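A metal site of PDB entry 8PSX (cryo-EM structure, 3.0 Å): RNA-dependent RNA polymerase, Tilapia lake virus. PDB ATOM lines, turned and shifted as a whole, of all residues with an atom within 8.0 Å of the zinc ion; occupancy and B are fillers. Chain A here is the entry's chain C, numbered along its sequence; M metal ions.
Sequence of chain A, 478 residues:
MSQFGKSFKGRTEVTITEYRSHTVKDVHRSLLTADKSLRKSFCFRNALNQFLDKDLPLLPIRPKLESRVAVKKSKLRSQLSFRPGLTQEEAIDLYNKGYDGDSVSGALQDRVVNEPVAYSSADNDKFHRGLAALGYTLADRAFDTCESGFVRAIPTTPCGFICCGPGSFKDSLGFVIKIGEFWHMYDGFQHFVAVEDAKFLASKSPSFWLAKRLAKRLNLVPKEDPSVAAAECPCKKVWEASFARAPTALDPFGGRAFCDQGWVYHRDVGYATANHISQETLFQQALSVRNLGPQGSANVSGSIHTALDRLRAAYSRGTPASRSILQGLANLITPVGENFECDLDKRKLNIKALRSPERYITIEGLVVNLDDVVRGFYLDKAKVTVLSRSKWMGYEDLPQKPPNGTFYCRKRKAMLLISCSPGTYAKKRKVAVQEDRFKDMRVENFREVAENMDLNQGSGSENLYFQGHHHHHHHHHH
Of the 23 residues printed, 4 come within 4 Å of the zinc ion.
Along chain A the residues within 4 Å of the zinc ion span positions 146 to 164.
The zinc ion is bound by SG of Cys 163 (2.3 Å), SG of Cys 146 (2.3 Å), SG of Cys 159 (2.3 Å) and SG of Cys 164 (2.3 Å).
The backbone carbonyl oxygen (O) of Cys 163 sits at hydrogen-bond distance from the guanidinium group (NE) of Arg 245, 2.6 Å away.
The side-chain amino group of Lys 170 sits close to the side-chain sulfur of Cys 146, 3.2 Å away.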
ATOM      1  N   ASP A 144      11.783 -23.815  21.397  1.00  0.00           N
ATOM      2  CA  ASP A 144      13.194 -23.770  21.760  1.00  0.00           C
ATOM      3  C   ASP A 144      13.838 -22.484  21.260  1.00  0.00           C
ATOM      4  O   ASP A 144      13.526 -22.007  20.168  1.00  0.00           O
ATOM      5  CB  ASP A 144      13.920 -24.991  21.193  1.00  0.00           C
ATOM      6  CG  ASP A 144      13.733 -25.154  19.709  1.00  0.00           C
ATOM      7  OD1 ASP A 144      12.570 -25.306  19.268  1.00  0.00           O
ATOM      8  OD2 ASP A 144      14.738 -25.133  18.965  1.00  0.00           O
ATOM      9  N   THR A 145      14.744 -21.929  22.065  1.00  0.00           N
ATOM     10  CA  THR A 145      15.419 -20.700  21.673  1.00  0.00           C
ATOM     11  C   THR A 145      16.184 -20.866  20.370  1.00  0.00           C
ATOM     12  O   THR A 145      16.290 -19.910  19.592  1.00  0.00           O
ATOM     13  CB  THR A 145      16.378 -20.248  22.785  1.00  0.00           C
ATOM     14  OG1 THR A 145      17.382 -21.246  22.984  1.00  0.00           O
ATOM     15  CG2 THR A 145      15.630 -20.011  24.083  1.00  0.00           C
ATOM     16  N   CYS A 146      16.719 -22.059  20.121  1.00  0.00           N
ATOM     17  CA  CYS A 146      17.487 -22.278  18.905  1.00  0.00           C
ATOM     18  C   CYS A 146      16.620 -22.139  17.660  1.00  0.00           C
ATOM     19  O   CYS A 146      17.037 -21.530  16.669  1.00  0.00           O
ATOM     20  CB  CYS A 146      18.138 -23.657  18.958  1.00  0.00           C
ATOM     21  SG  CYS A 146      19.667 -23.788  18.020  1.00  0.00           S
ATOM     22  N   GLU A 147      15.403 -22.692  17.699  1.00  0.00           N
ATOM     23  CA  GLU A 147      14.500 -22.580  16.560  1.00  0.00           C
ATOM     24  C   GLU A 147      14.131 -21.118  16.308  1.00  0.00           C
ATOM     25  O   GLU A 147      14.075 -20.677  15.154  1.00  0.00           O
ATOM     26  CB  GLU A 147      13.249 -23.416  16.815  1.00  0.00           C
ATOM     27  CG  GLU A 147      12.240 -23.400  15.666  1.00  0.00           C
ATOM     28  CD  GLU A 147      10.802 -23.350  16.154  1.00  0.00           C
ATOM     29  OE1 GLU A 147      10.566 -23.617  17.354  1.00  0.00           O
ATOM     30  OE2 GLU A 147       9.916 -23.036  15.343  1.00  0.00           O
ATOM     31  N   SER A 148      13.878 -20.360  17.375  1.00  0.00           N
ATOM     32  CA  SER A 148      13.554 -18.948  17.214  1.00  0.00           C
ATOM     33  C   SER A 148      14.744 -18.180  16.644  1.00  0.00           C
ATOM     34  O   SER A 148      14.562 -17.253  15.849  1.00  0.00           O
ATOM     35  CB  SER A 148      13.114 -18.353  18.542  1.00  0.00           C
ATOM     36  OG  SER A 148      13.805 -18.955  19.621  1.00  0.00           O
ATOM     37  N   GLY A 149      15.956 -18.526  17.058  1.00  0.00           N
ATOM     38  CA  GLY A 149      17.134 -17.855  16.548  1.00  0.00           C
ATOM     39  C   GLY A 149      17.487 -18.205  15.123  1.00  0.00           C
ATOM     40  O   GLY A 149      18.101 -17.385  14.421  1.00  0.00           O
ATOM     41  N   PHE A 150      17.108 -19.403  14.660  1.00  0.00           N
ATOM     42  CA  PHE A 150      17.396 -19.785  13.283  1.00  0.00           C
ATOM     43  C   PHE A 150      16.664 -18.902  12.292  1.00  0.00           C
ATOM     44  O   PHE A 150      17.226 -18.493  11.269  1.00  0.00           O
ATOM     45  CB  PHE A 150      17.037 -21.259  13.073  1.00  0.00           C
ATOM     46  CG  PHE A 150      17.368 -21.765  11.697  1.00  0.00           C
ATOM     47  CD1 PHE A 150      18.679 -21.770  11.239  1.00  0.00           C
ATOM     48  CD2 PHE A 150      16.375 -22.259  10.866  1.00  0.00           C
ATOM     49  CE1 PHE A 150      18.985 -22.243   9.980  1.00  0.00           C
ATOM     50  CE2 PHE A 150      16.681 -22.733   9.607  1.00  0.00           C
ATOM     51  CZ  PHE A 150      17.982 -22.722   9.164  1.00  0.00           C
ATOM     52  N   PRO A 155      20.200 -13.024  15.333  1.00  0.00           N
ATOM     53  CA  PRO A 155      19.783 -13.644  16.587  1.00  0.00           C
ATOM     54  C   PRO A 155      20.264 -12.860  17.801  1.00  0.00           C
ATOM     55  O   PRO A 155      21.371 -12.311  17.807  1.00  0.00           O
ATOM     56  CB  PRO A 155      20.436 -15.036  16.528  1.00  0.00           C
ATOM     57  CG  PRO A 155      20.790 -15.253  15.087  1.00  0.00           C
ATOM     58  CD  PRO A 155      21.071 -13.901  14.536  1.00  0.00           C
ATOM     59  N   THR A 157      20.605 -14.193  20.981  1.00  0.00           N
ATOM     60  CA  THR A 157      21.470 -15.054  21.796  1.00  0.00           C
ATOM     61  C   THR A 157      22.180 -16.075  20.917  1.00  0.00           C
ATOM     62  O   THR A 157      21.575 -17.098  20.557  1.00  0.00           O
ATOM     63  CB  THR A 157      20.654 -15.764  22.878  1.00  0.00           C
ATOM     64  OG1 THR A 157      19.665 -16.592  22.267  1.00  0.00           O
ATOM     65  CG2 THR A 157      19.979 -14.757  23.786  1.00  0.00           C
ATOM     66  N   PRO A 158      23.434 -15.847  20.529  1.00  0.00           N
ATOM     67  CA  PRO A 158      24.174 -16.899  19.831  1.00  0.00           C
ATOM     68  C   PRO A 158      24.387 -18.111  20.738  1.00  0.00           C
ATOM     69  O   PRO A 158      24.564 -17.979  21.945  1.00  0.00           O
ATOM     70  CB  PRO A 158      25.502 -16.228  19.468  1.00  0.00           C
ATOM     71  CG  PRO A 158      25.625 -15.081  20.409  1.00  0.00           C
ATOM     72  CD  PRO A 158      24.234 -14.620  20.686  1.00  0.00           C
ATOM     73  N   CYS A 159      24.347 -19.300  20.128  1.00  0.00           N
ATOM     74  CA  CYS A 159      24.520 -20.544  20.861  1.00  0.00           C
ATOM     75  C   CYS A 159      25.761 -21.323  20.419  1.00  0.00           C
ATOM     76  O   CYS A 159      25.843 -22.523  20.662  1.00  0.00           O
ATOM     77  CB  CYS A 159      23.269 -21.427  20.716  1.00  0.00           C
ATOM     78  SG  CYS A 159      23.137 -22.305  19.137  1.00  0.00           S
ATOM     79  N   GLY A 160      26.714 -20.647  19.770  1.00  0.00           N
ATOM     80  CA  GLY A 160      27.961 -21.294  19.407  1.00  0.00           C
ATOM     81  C   GLY A 160      27.858 -22.277  18.260  1.00  0.00           C
ATOM     82  O   GLY A 160      28.702 -23.179  18.165  1.00  0.00           O
ATOM     83  N   PHE A 161      26.861 -22.147  17.387  1.00  0.00           N
ATOM     84  CA  PHE A 161      26.687 -23.047  16.266  1.00  0.00           C
ATOM     85  C   PHE A 161      26.234 -22.239  15.051  1.00  0.00           C
ATOM     86  O   PHE A 161      25.968 -21.038  15.137  1.00  0.00           O
ATOM     87  CB  PHE A 161      25.689 -24.160  16.606  1.00  0.00           C
ATOM     88  CG  PHE A 161      26.242 -25.189  17.556  1.00  0.00           C
ATOM     89  CD1 PHE A 161      27.243 -26.050  17.155  1.00  0.00           C
ATOM     90  CD2 PHE A 161      25.759 -25.285  18.845  1.00  0.00           C
ATOM     91  CE1 PHE A 161      27.754 -26.995  18.027  1.00  0.00           C
ATOM     92  CE2 PHE A 161      26.262 -26.223  19.718  1.00  0.00           C
ATOM     93  CZ  PHE A 161      27.264 -27.081  19.308  1.00  0.00           C
ATOM     94  N   ILE A 162      26.147 -22.927  13.905  1.00  0.00           N
ATOM     95  CA  ILE A 162      25.835 -22.256  12.649  1.00  0.00           C
ATOM     96  C   ILE A 162      24.454 -21.631  12.676  1.00  0.00           C
ATOM     97  O   ILE A 162      24.225 -20.577  12.084  1.00  0.00           O
ATOM     98  CB  ILE A 162      25.977 -23.249  11.470  1.00  0.00           C
ATOM     99  CG1 ILE A 162      25.964 -22.495  10.144  1.00  0.00           C
ATOM    100  CG2 ILE A 162      24.870 -24.282  11.513  1.00  0.00           C
ATOM    101  CD1 ILE A 162      26.781 -23.161   9.057  1.00  0.00           C
ATOM    102  N   CYS A 163      23.502 -22.266  13.361  1.00  0.00           N
ATOM    103  CA  CYS A 163      22.110 -21.829  13.321  1.00  0.00           C
ATOM    104  C   CYS A 163      21.959 -20.389  13.809  1.00  0.00           C
ATOM    105  O   CYS A 163      21.239 -19.599  13.189  1.00  0.00           O
ATOM    106  CB  CYS A 163      21.259 -22.775  14.166  1.00  0.00           C
ATOM    107  SG  CYS A 163      22.124 -23.295  15.658  1.00  0.00           S
ATOM    108  N   CYS A 164      22.621 -20.041  14.898  1.00  0.00           N
ATOM    109  CA  CYS A 164      22.460 -18.735  15.528  1.00  0.00           C
ATOM    110  C   CYS A 164      23.711 -17.866  15.434  1.00  0.00           C
ATOM    111  O   CYS A 164      23.772 -16.826  16.088  1.00  0.00           O
ATOM    112  CB  CYS A 164      22.046 -18.910  16.995  1.00  0.00           C
ATOM    113  SG  CYS A 164      20.690 -20.084  17.240  1.00  0.00           S
ATOM    114  N   GLY A 165      24.691 -18.267  14.644  1.00  0.00           N
ATOM    115  CA  GLY A 165      25.905 -17.507  14.487  1.00  0.00           C
ATOM    116  C   GLY A 165      26.995 -18.329  13.829  1.00  0.00           C
ATOM    117  O   GLY A 165      26.766 -19.464  13.397  1.00  0.00           O
ATOM    118  N   SER A 168      29.936 -24.499  13.995  1.00  0.00           N
ATOM    119  CA  SER A 168      29.711 -25.787  13.381  1.00  0.00           C
ATOM    120  C   SER A 168      28.230 -26.137  13.435  1.00  0.00           C
ATOM    121  O   SER A 168      27.380 -25.306  13.749  1.00  0.00           O
ATOM    122  CB  SER A 168      30.573 -26.854  14.058  1.00  0.00           C
ATOM    123  OG  SER A 168      30.811 -27.948  13.189  1.00  0.00           O
ATOM    124  N   LYS A 170      24.841 -27.989  14.744  1.00  0.00           N
ATOM    125  CA  LYS A 170      24.154 -28.570  15.879  1.00  0.00           C
ATOM    126  C   LYS A 170      23.508 -29.893  15.483  1.00  0.00           C
ATOM    127  O   LYS A 170      23.459 -30.264  14.304  1.00  0.00           O
ATOM    128  CB  LYS A 170      23.099 -27.586  16.406  1.00  0.00           C
ATOM    129  CG  LYS A 170      22.622 -27.842  17.830  1.00  0.00           C
ATOM    130  CD  LYS A 170      21.561 -26.831  18.238  1.00  0.00           C
ATOM    131  CE  LYS A 170      20.757 -27.329  19.428  1.00  0.00           C
ATOM    132  NZ  LYS A 170      19.680 -26.380  19.814  1.00  0.00           N
ATOM    133  N   SER A 172      20.337 -30.826  15.550  1.00  0.00           N
ATOM    134  CA  SER A 172      19.065 -30.731  14.851  1.00  0.00           C
ATOM    135  C   SER A 172      19.184 -30.148  13.450  1.00  0.00           C
ATOM    136  O   SER A 172      18.191 -30.135  12.716  1.00  0.00           O
ATOM    137  CB  SER A 172      18.075 -29.892  15.659  1.00  0.00           C
ATOM    138  OG  SER A 172      18.726 -28.783  16.256  1.00  0.00           O
ATOM    139  N   LEU A 173      20.351 -29.665  13.042  1.00  0.00           N
ATOM    140  CA  LEU A 173      20.526 -29.012  11.754  1.00  0.00           C
ATOM    141  C   LEU A 173      21.054 -30.005  10.725  1.00  0.00           C
ATOM    142  O   LEU A 173      22.047 -30.690  10.973  1.00  0.00           O
ATOM    143  CB  LEU A 173      21.490 -27.828  11.863  1.00  0.00           C
ATOM    144  CG  LEU A 173      21.231 -26.880  13.030  1.00  0.00           C
ATOM    145  CD1 LEU A 173      22.349 -25.852  13.113  1.00  0.00           C
ATOM    146  CD2 LEU A 173      19.881 -26.196  12.878  1.00  0.00           C
ATOM    147  N   ARG A 245      27.802 -17.209   9.309  1.00  0.00           N
ATOM    148  CA  ARG A 245      26.352 -17.136   9.155  1.00  0.00           C
ATOM    149  C   ARG A 245      26.001 -15.770   8.583  1.00  0.00           C
ATOM    150  O   ARG A 245      26.184 -14.745   9.249  1.00  0.00           O
ATOM    151  CB  ARG A 245      25.646 -17.361  10.492  1.00  0.00           C
ATOM    152  CG  ARG A 245      24.135 -17.302  10.404  1.00  0.00           C
ATOM    153  CD  ARG A 245      23.510 -17.311  11.791  1.00  0.00           C
ATOM    154  NE  ARG A 245      22.070 -17.539  11.764  1.00  0.00           N
ATOM    155  CZ  ARG A 245      21.166 -16.597  11.518  1.00  0.00           C
ATOM    156  NH1 ARG A 245      21.519 -15.357  11.218  1.00  0.00           N
ATOM    157  NH2 ARG A 245      19.882 -16.911  11.565  1.00  0.00           N
ATOM    158  N   HIS A 266      16.549 -26.694   9.271  1.00  0.00           N
ATOM    159  CA  HIS A 266      16.181 -27.026  10.642  1.00  0.00           C
ATOM    160  C   HIS A 266      14.907 -27.851  10.644  1.00  0.00           C
ATOM    161  O   HIS A 266      13.968 -27.553   9.888  1.00  0.00           O
ATOM    162  CB  HIS A 266      16.006 -25.765  11.479  1.00  0.00           C
ATOM    163  CG  HIS A 266      15.952 -26.016  12.961  1.00  0.00           C
ATOM    164  ND1 HIS A 266      14.908 -26.678  13.567  1.00  0.00           N
ATOM    165  CD2 HIS A 266      16.815 -25.681  13.950  1.00  0.00           C
ATOM    166  CE1 HIS A 266      15.126 -26.747  14.864  1.00  0.00           C
ATOM    167  NE2 HIS A 266      16.281 -26.148  15.125  1.00  0.00           N
HETATM  168 ZN    ZN M   1      21.384 -22.279  17.608  1.00  0.00          ZN
